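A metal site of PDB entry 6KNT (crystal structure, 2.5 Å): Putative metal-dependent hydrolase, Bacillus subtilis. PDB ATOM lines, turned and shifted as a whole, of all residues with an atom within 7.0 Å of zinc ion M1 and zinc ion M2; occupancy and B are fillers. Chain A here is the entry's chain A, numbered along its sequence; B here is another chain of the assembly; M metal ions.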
ATOM      1  N   TYR A  15      -2.549  13.267 -15.993  1.00  0.00           N
ATOM      2  CA  TYR A  15      -2.106  12.920 -17.342  1.00  0.00           C
ATOM      3  C   TYR A  15      -2.905  11.769 -17.945  1.00  0.00           C
ATOM      4  O   TYR A  15      -3.314  10.841 -17.216  1.00  0.00           O
ATOM      5  CB  TYR A  15      -0.619  12.583 -17.347  1.00  0.00           C
ATOM      6  CG  TYR A  15       0.219  13.816 -17.511  1.00  0.00           C
ATOM      7  CD1 TYR A  15       0.612  14.256 -18.786  1.00  0.00           C
ATOM      8  CD2 TYR A  15       0.585  14.592 -16.397  1.00  0.00           C
ATOM      9  CE1 TYR A  15       1.379  15.394 -18.946  1.00  0.00           C
ATOM     10  CE2 TYR A  15       1.314  15.739 -16.544  1.00  0.00           C
ATOM     11  CZ  TYR A  15       1.719  16.144 -17.798  1.00  0.00           C
ATOM     12  OH  TYR A  15       2.460  17.289 -17.925  1.00  0.00           O
ATOM     13  N   GLY A  16      -3.125  11.829 -19.259  1.00  0.00           N
ATOM     14  CA  GLY A  16      -3.694  10.728 -20.001  1.00  0.00           C
ATOM     15  C   GLY A  16      -2.744   9.582 -20.337  1.00  0.00           C
ATOM     16  O   GLY A  16      -1.568   9.780 -20.716  1.00  0.00           O
ATOM     17  N   GLY A  17      -3.257   8.357 -20.231  1.00  0.00           N
ATOM     18  CA  GLY A  17      -2.563   7.188 -20.747  1.00  0.00           C
ATOM     19  C   GLY A  17      -1.503   6.691 -19.786  1.00  0.00           C
ATOM     20  O   GLY A  17      -1.559   5.552 -19.335  1.00  0.00           O
ATOM     21  N   SER A  26      -4.950   9.734 -13.960  1.00  0.00           N
ATOM     22  CA  SER A  26      -6.207  10.139 -13.325  1.00  0.00           C
ATOM     23  C   SER A  26      -6.379   9.733 -11.874  1.00  0.00           C
ATOM     24  O   SER A  26      -6.413   8.536 -11.550  1.00  0.00           O
ATOM     25  CB  SER A  26      -7.375   9.598 -14.142  1.00  0.00           C
ATOM     26  OG  SER A  26      -7.410  10.210 -15.417  1.00  0.00           O
ATOM     27  N   ASP A  40     -11.108   7.680  -9.342  1.00  0.00           N
ATOM     28  CA  ASP A  40     -10.090   7.079 -10.184  1.00  0.00           C
ATOM     29  C   ASP A  40      -8.729   6.940  -9.456  1.00  0.00           C
ATOM     30  O   ASP A  40      -8.452   7.665  -8.494  1.00  0.00           O
ATOM     31  CB  ASP A  40      -9.974   7.806 -11.525  1.00  0.00           C
ATOM     32  CG  ASP A  40     -11.108   7.426 -12.486  1.00  0.00           C
ATOM     33  OD1 ASP A  40     -11.880   6.464 -12.162  1.00  0.00           O
ATOM     34  OD2 ASP A  40     -11.212   8.073 -13.572  1.00  0.00           O
ATOM     35  N   SER A  64     -14.273   5.315 -12.788  1.00  0.00           N
ATOM     36  CA  SER A  64     -15.100   5.605 -13.945  1.00  0.00           C
ATOM     37  C   SER A  64     -15.094   4.450 -14.943  1.00  0.00           C
ATOM     38  O   SER A  64     -16.102   4.173 -15.604  1.00  0.00           O
ATOM     39  CB  SER A  64     -14.647   6.902 -14.612  1.00  0.00           C
ATOM     40  OG  SER A  64     -13.367   6.761 -15.172  1.00  0.00           O
ATOM     41  N   HIS A  65     -13.944   3.801 -15.062  1.00  0.00           N
ATOM     42  CA  HIS A  65     -13.759   2.709 -16.028  1.00  0.00           C
ATOM     43  C   HIS A  65     -12.444   1.970 -15.784  1.00  0.00           C
ATOM     44  O   HIS A  65     -11.598   2.432 -15.000  1.00  0.00           O
ATOM     45  CB  HIS A  65     -13.903   3.199 -17.484  1.00  0.00           C
ATOM     46  CG  HIS A  65     -12.791   4.080 -17.988  1.00  0.00           C
ATOM     47  ND1 HIS A  65     -12.497   5.314 -17.432  1.00  0.00           N
ATOM     48  CD2 HIS A  65     -11.971   3.948 -19.058  1.00  0.00           C
ATOM     49  CE1 HIS A  65     -11.517   5.883 -18.117  1.00  0.00           C
ATOM     50  NE2 HIS A  65     -11.178   5.073 -19.109  1.00  0.00           N
ATOM     51  N   TYR A  66     -12.249   0.849 -16.457  1.00  0.00           N
ATOM     52  CA  TYR A  66     -11.141  -0.017 -16.111  1.00  0.00           C
ATOM     53  C   TYR A  66      -9.986   0.077 -17.079  1.00  0.00           C
ATOM     54  O   TYR A  66      -9.397  -0.929 -17.425  1.00  0.00           O
ATOM     55  CB  TYR A  66     -11.619  -1.457 -15.957  1.00  0.00           C
ATOM     56  CG  TYR A  66     -12.691  -1.617 -14.914  1.00  0.00           C
ATOM     57  CD1 TYR A  66     -12.391  -1.468 -13.559  1.00  0.00           C
ATOM     58  CD2 TYR A  66     -14.007  -1.889 -15.276  1.00  0.00           C
ATOM     59  CE1 TYR A  66     -13.380  -1.625 -12.584  1.00  0.00           C
ATOM     60  CE2 TYR A  66     -14.996  -2.028 -14.310  1.00  0.00           C
ATOM     61  CZ  TYR A  66     -14.671  -1.888 -12.970  1.00  0.00           C
ATOM     62  OH  TYR A  66     -15.645  -2.026 -12.002  1.00  0.00           O
ATOM     63  N   HIS A  67      -9.647   1.287 -17.516  1.00  0.00           N
ATOM     64  CA  HIS A  67      -8.425   1.451 -18.299  1.00  0.00           C
ATOM     65  C   HIS A  67      -7.280   1.594 -17.315  1.00  0.00           C
ATOM     66  O   HIS A  67      -7.470   2.152 -16.226  1.00  0.00           O
ATOM     67  CB  HIS A  67      -8.521   2.667 -19.225  1.00  0.00           C
ATOM     68  CG  HIS A  67      -8.998   2.340 -20.615  1.00  0.00           C
ATOM     69  ND1 HIS A  67      -9.538   3.297 -21.459  1.00  0.00           N
ATOM     70  CD2 HIS A  67      -9.044   1.175 -21.292  1.00  0.00           C
ATOM     71  CE1 HIS A  67      -9.860   2.726 -22.609  1.00  0.00           C
ATOM     72  NE2 HIS A  67      -9.571   1.441 -22.528  1.00  0.00           N
ATOM     73  N   HIS A  68      -6.091   1.113 -17.694  1.00  0.00           N
ATOM     74  CA  HIS A  68      -4.913   1.106 -16.842  1.00  0.00           C
ATOM     75  C   HIS A  68      -4.664   2.432 -16.158  1.00  0.00           C
ATOM     76  O   HIS A  68      -4.264   2.475 -14.995  1.00  0.00           O
ATOM     77  CB  HIS A  68      -3.646   0.745 -17.629  1.00  0.00           C
ATOM     78  CG  HIS A  68      -3.688  -0.611 -18.261  1.00  0.00           C
ATOM     79  ND1 HIS A  68      -4.061  -1.749 -17.583  1.00  0.00           N
ATOM     80  CD2 HIS A  68      -3.367  -1.005 -19.518  1.00  0.00           C
ATOM     81  CE1 HIS A  68      -3.976  -2.785 -18.387  1.00  0.00           C
ATOM     82  NE2 HIS A  68      -3.547  -2.367 -19.571  1.00  0.00           N
ATOM     83  N   ASP A  69      -4.817   3.523 -16.897  1.00  0.00           N
ATOM     84  CA  ASP A  69      -4.508   4.818 -16.355  1.00  0.00           C
ATOM     85  C   ASP A  69      -5.569   5.328 -15.367  1.00  0.00           C
ATOM     86  O   ASP A  69      -5.389   6.371 -14.779  1.00  0.00           O
ATOM     87  CB  ASP A  69      -4.183   5.829 -17.452  1.00  0.00           C
ATOM     88  CG  ASP A  69      -5.286   5.926 -18.556  1.00  0.00           C
ATOM     89  OD1 ASP A  69      -5.900   4.887 -18.991  1.00  0.00           O
ATOM     90  OD2 ASP A  69      -5.502   7.100 -18.971  1.00  0.00           O
ATOM     91  N   HIS A  70      -6.624   4.558 -15.140  1.00  0.00           N
ATOM     92  CA  HIS A  70      -7.572   4.878 -14.071  1.00  0.00           C
ATOM     93  C   HIS A  70      -7.576   3.867 -12.915  1.00  0.00           C
ATOM     94  O   HIS A  70      -8.251   4.119 -11.882  1.00  0.00           O
ATOM     95  CB  HIS A  70      -9.009   5.130 -14.613  1.00  0.00           C
ATOM     96  CG  HIS A  70      -9.049   6.209 -15.642  1.00  0.00           C
ATOM     97  ND1 HIS A  70      -9.590   7.459 -15.409  1.00  0.00           N
ATOM     98  CD2 HIS A  70      -8.501   6.278 -16.878  1.00  0.00           C
ATOM     99  CE1 HIS A  70      -9.416   8.231 -16.463  1.00  0.00           C
ATOM    100  NE2 HIS A  70      -8.751   7.541 -17.362  1.00  0.00           N
ATOM    101  N   HIS A 140     -16.507   5.996 -25.344  1.00  0.00           N
ATOM    102  CA  HIS A 140     -15.113   5.642 -25.088  1.00  0.00           C
ATOM    103  C   HIS A 140     -15.073   4.172 -25.497  1.00  0.00           C
ATOM    104  O   HIS A 140     -16.138   3.556 -25.582  1.00  0.00           O
ATOM    105  CB  HIS A 140     -14.791   5.825 -23.601  1.00  0.00           C
ATOM    106  CG  HIS A 140     -13.331   5.888 -23.255  1.00  0.00           C
ATOM    107  ND1 HIS A 140     -12.463   6.816 -23.804  1.00  0.00           N
ATOM    108  CD2 HIS A 140     -12.583   5.179 -22.367  1.00  0.00           C
ATOM    109  CE1 HIS A 140     -11.250   6.633 -23.307  1.00  0.00           C
ATOM    110  NE2 HIS A 140     -11.297   5.654 -22.419  1.00  0.00           N
ATOM    111  N   PRO A 141     -13.881   3.597 -25.794  1.00  0.00           N
ATOM    112  CA  PRO A 141     -13.910   2.213 -26.327  1.00  0.00           C
ATOM    113  C   PRO A 141     -14.231   1.138 -25.284  1.00  0.00           C
ATOM    114  O   PRO A 141     -14.476  -0.004 -25.637  1.00  0.00           O
ATOM    115  CB  PRO A 141     -12.501   1.986 -26.907  1.00  0.00           C
ATOM    116  CG  PRO A 141     -11.838   3.306 -26.947  1.00  0.00           C
ATOM    117  CD  PRO A 141     -12.562   4.231 -25.949  1.00  0.00           C
ATOM    118  N   VAL A 142     -14.190   1.493 -23.997  1.00  0.00           N
ATOM    119  CA  VAL A 142     -14.719   0.604 -22.945  1.00  0.00           C
ATOM    120  C   VAL A 142     -15.857   1.309 -22.221  1.00  0.00           C
ATOM    121  O   VAL A 142     -15.974   2.551 -22.256  1.00  0.00           O
ATOM    122  CB  VAL A 142     -13.598   0.113 -21.968  1.00  0.00           C
ATOM    123  CG1 VAL A 142     -12.507  -0.661 -22.744  1.00  0.00           C
ATOM    124  CG2 VAL A 142     -12.977   1.287 -21.166  1.00  0.00           C
ATOM    125  N   CYS A 144     -17.742   3.223 -19.633  1.00  0.00           N
ATOM    126  CA  CYS A 144     -17.182   4.309 -18.835  1.00  0.00           C
ATOM    127  C   CYS A 144     -18.282   5.307 -18.432  1.00  0.00           C
ATOM    128  O   CYS A 144     -19.200   5.561 -19.213  1.00  0.00           O
ATOM    129  CB  CYS A 144     -16.094   5.033 -19.641  1.00  0.00           C
ATOM    130  SG  CYS A 144     -15.250   6.422 -18.751  1.00  0.00           S
ATOM    131  N   TYR A 158     -17.353  15.470 -13.393  1.00  0.00           N
ATOM    132  CA  TYR A 158     -16.155  14.891 -13.937  1.00  0.00           C
ATOM    133  C   TYR A 158     -16.589  14.109 -15.198  1.00  0.00           C
ATOM    134  O   TYR A 158     -17.504  13.257 -15.113  1.00  0.00           O
ATOM    135  CB  TYR A 158     -15.569  13.965 -12.898  1.00  0.00           C
ATOM    136  CG  TYR A 158     -14.433  13.068 -13.365  1.00  0.00           C
ATOM    137  CD1 TYR A 158     -13.351  13.584 -14.052  1.00  0.00           C
ATOM    138  CD2 TYR A 158     -14.442  11.687 -13.068  1.00  0.00           C
ATOM    139  CE1 TYR A 158     -12.298  12.757 -14.459  1.00  0.00           C
ATOM    140  CE2 TYR A 158     -13.397  10.862 -13.428  1.00  0.00           C
ATOM    141  CZ  TYR A 158     -12.328  11.395 -14.127  1.00  0.00           C
ATOM    142  OH  TYR A 158     -11.280  10.581 -14.509  1.00  0.00           O
ATOM    143  N   ALA A 160     -14.915  12.006 -16.831  1.00  0.00           N
ATOM    144  CA  ALA A 160     -14.115  10.804 -17.075  1.00  0.00           C
ATOM    145  C   ALA A 160     -13.634  10.862 -18.553  1.00  0.00           C
ATOM    146  O   ALA A 160     -13.370  11.960 -19.083  1.00  0.00           O
ATOM    147  CB  ALA A 160     -14.932   9.521 -16.767  1.00  0.00           C
ATOM    148  N   ASP A 161     -13.525   9.712 -19.227  1.00  0.00           N
ATOM    149  CA  ASP A 161     -13.009   9.689 -20.597  1.00  0.00           C
ATOM    150  C   ASP A 161     -14.155   9.603 -21.580  1.00  0.00           C
ATOM    151  O   ASP A 161     -15.037   8.736 -21.432  1.00  0.00           O
ATOM    152  CB  ASP A 161     -12.075   8.487 -20.826  1.00  0.00           C
ATOM    153  CG  ASP A 161     -10.715   8.679 -20.201  1.00  0.00           C
ATOM    154  OD1 ASP A 161     -10.544   9.531 -19.310  1.00  0.00           O
ATOM    155  OD2 ASP A 161      -9.794   7.962 -20.650  1.00  0.00           O
ATOM    156  N   SER A 162     -14.131  10.454 -22.606  1.00  0.00           N
ATOM    157  CA  SER A 162     -15.176  10.442 -23.610  1.00  0.00           C
ATOM    158  C   SER A 162     -14.835  11.251 -24.856  1.00  0.00           C
ATOM    159  O   SER A 162     -14.078  12.224 -24.791  1.00  0.00           O
ATOM    160  CB  SER A 162     -16.460  11.058 -23.027  1.00  0.00           C
ATOM    161  OG  SER A 162     -17.560  10.898 -23.930  1.00  0.00           O
ATOM    162  N   GLU A 181     -12.057  16.076 -19.514  1.00  0.00           N
ATOM    163  CA  GLU A 181     -10.905  15.529 -20.173  1.00  0.00           C
ATOM    164  C   GLU A 181     -10.659  16.420 -21.382  1.00  0.00           C
ATOM    165  O   GLU A 181     -11.598  17.038 -21.924  1.00  0.00           O
ATOM    166  CB  GLU A 181     -11.132  14.084 -20.628  1.00  0.00           C
ATOM    167  CG  GLU A 181     -12.026  13.890 -21.897  1.00  0.00           C
ATOM    168  CD  GLU A 181     -11.367  12.999 -22.901  1.00  0.00           C
ATOM    169  OE1 GLU A 181     -10.687  13.527 -23.805  1.00  0.00           O
ATOM    170  OE2 GLU A 181     -11.478  11.752 -22.792  1.00  0.00           O
ATOM    171  N   ASN A 183      -7.778  15.530 -23.931  1.00  0.00           N
ATOM    172  CA  ASN A 183      -6.620  14.841 -24.473  1.00  0.00           C
ATOM    173  C   ASN A 183      -6.099  15.432 -25.814  1.00  0.00           C
ATOM    174  O   ASN A 183      -4.958  15.172 -26.206  1.00  0.00           O
ATOM    175  CB  ASN A 183      -6.886  13.335 -24.595  1.00  0.00           C
ATOM    176  CG  ASN A 183      -5.650  12.485 -24.290  1.00  0.00           C
ATOM    177  OD1 ASN A 183      -4.581  12.728 -24.809  1.00  0.00           O
ATOM    178  ND2 ASN A 183      -5.817  11.456 -23.446  1.00  0.00           N
ATOM    179  N   ALA A 193     -10.340   7.881 -30.803  1.00  0.00           N
ATOM    180  CA  ALA A 193      -9.786   7.439 -29.534  1.00  0.00           C
ATOM    181  C   ALA A 193     -10.788   7.537 -28.356  1.00  0.00           C
ATOM    182  O   ALA A 193     -10.493   7.061 -27.245  1.00  0.00           O
ATOM    183  CB  ALA A 193      -8.490   8.194 -29.222  1.00  0.00           C
ATOM    184  N   GLY A 194     -11.956   8.126 -28.590  1.00  0.00           N
ATOM    185  CA  GLY A 194     -12.911   8.365 -27.504  1.00  0.00           C
ATOM    186  C   GLY A 194     -12.453   9.490 -26.576  1.00  0.00           C
ATOM    187  O   GLY A 194     -12.438   9.311 -25.341  1.00  0.00           O
ATOM    188  N   HIS A 195     -12.062  10.628 -27.144  1.00  0.00           N
ATOM    189  CA  HIS A 195     -11.536  11.760 -26.370  1.00  0.00           C
ATOM    190  C   HIS A 195     -12.055  13.090 -26.930  1.00  0.00           C
ATOM    191  O   HIS A 195     -12.570  13.167 -28.072  1.00  0.00           O
ATOM    192  CB  HIS A 195      -9.975  11.788 -26.360  1.00  0.00           C
ATOM    193  CG  HIS A 195      -9.365  10.731 -25.483  1.00  0.00           C
ATOM    194  ND1 HIS A 195      -9.757  10.534 -24.174  1.00  0.00           N
ATOM    195  CD2 HIS A 195      -8.427   9.794 -25.745  1.00  0.00           C
ATOM    196  CE1 HIS A 195      -9.053   9.532 -23.658  1.00  0.00           C
ATOM    197  NE2 HIS A 195      -8.253   9.064 -24.594  1.00  0.00           N
ATOM    198  N   HIS A 217      -6.737  15.012 -18.067  1.00  0.00           N
ATOM    199  CA  HIS A 217      -6.363  13.903 -18.958  1.00  0.00           C
ATOM    200  C   HIS A 217      -5.433  14.421 -20.112  1.00  0.00           C
ATOM    201  O   HIS A 217      -5.641  14.133 -21.311  1.00  0.00           O
ATOM    202  CB  HIS A 217      -7.619  13.239 -19.522  1.00  0.00           C
ATOM    203  CG  HIS A 217      -7.478  11.779 -19.814  1.00  0.00           C
ATOM    204  ND1 HIS A 217      -6.998  11.301 -21.021  1.00  0.00           N
ATOM    205  CD2 HIS A 217      -7.764  10.694 -19.068  1.00  0.00           C
ATOM    206  CE1 HIS A 217      -7.020   9.979 -21.002  1.00  0.00           C
ATOM    207  NE2 HIS A 217      -7.491   9.584 -19.822  1.00  0.00           N
ATOM    208  N   PHE B  79       0.789   1.532 -22.355  1.00  0.00           N
ATOM    209  CA  PHE B  79       0.178   2.736 -22.906  1.00  0.00           C
ATOM    210  C   PHE B  79       1.211   3.799 -23.310  1.00  0.00           C
ATOM    211  O   PHE B  79       0.983   4.513 -24.260  1.00  0.00           O
ATOM    212  CB  PHE B  79      -0.854   3.358 -21.940  1.00  0.00           C
ATOM    213  CG  PHE B  79      -2.217   2.685 -21.951  1.00  0.00           C
ATOM    214  CD1 PHE B  79      -2.509   1.664 -22.856  1.00  0.00           C
ATOM    215  CD2 PHE B  79      -3.202   3.096 -21.059  1.00  0.00           C
ATOM    216  CE1 PHE B  79      -3.776   1.060 -22.853  1.00  0.00           C
ATOM    217  CE2 PHE B  79      -4.469   2.525 -21.058  1.00  0.00           C
ATOM    218  CZ  PHE B  79      -4.762   1.495 -21.958  1.00  0.00           C
HETATM  219 ZN    ZN M   1      -9.827   5.511 -20.931  1.00  0.00          ZN
HETATM  220 ZN    ZN M   2      -8.066   7.590 -19.463  1.00  0.00          ZN
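ND1 of His 65 is in hydrogen-bond range of OG of Ser 64, 2.8 Å away.
A ring nitrogen (ND1) of His 217 sits at hydrogen-bond distance from the side-chain amide nitrogen of Asn 183 (2.7 Å).
ND1 of His 140 lies within hydrogen-bond range of O of Gly 194 (2.9 Å).
The side-chain carboxylate (OD2) of Asp 40 sits at hydrogen-bond distance from a ring nitrogen (ND1) of His 70 (2.5 Å).
The backbone NH (N) of Ser 26 sits at hydrogen-bond distance from the backbone carbonyl oxygen (O) of Asp 69 (3.5 Å).
The side-chain carboxylate of Asp 69 is in hydrogen-bond range of the backbone NH of Gly 17.
A ring nitrogen (NE2) of His 217 sits close to the side-chain carboxylate (OD2) of Asp 69 (3.3 Å).
A ring nitrogen (ND1) of His 65 sits at hydrogen-bond distance from the side-chain sulfur of Cys 144 (3.2 Å).
Of the 27 residues printed, 4 come within 4 Å of zinc ion M1.
The nearest printed residue that does not touch zinc ion M1 is His 70 (4.2 Å).
Zinc ion M1 is bound by a ring nitrogen (NE2) of His 140, 2.1 Å away.
A ring nitrogen (ND1) of His 67 is bound to zinc ion M1 (2.3 Å).
Zinc ion M1 is bound by NE2 of His 65 (2.3 Å).
The side-chain carboxylate (OD2) of Asp 161 binds zinc ion M1, 2.5 Å away.
Zinc ion M1 has four donor atoms within binding distance.
Zinc ion M2 is bound by a ring nitrogen (NE2) of His 217 (2.1 Å), the side-chain carboxylate (OD2) of Asp 161 (2.1 Å) and a ring nitrogen (NE2) of His 70 (2.2 Å).
Zinc ion M2 has three donor atoms within binding distance.
Slightly farther from zinc ion M2 lies the side-chain carboxylate (OD2) of Asp 69 (2.7 Å).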
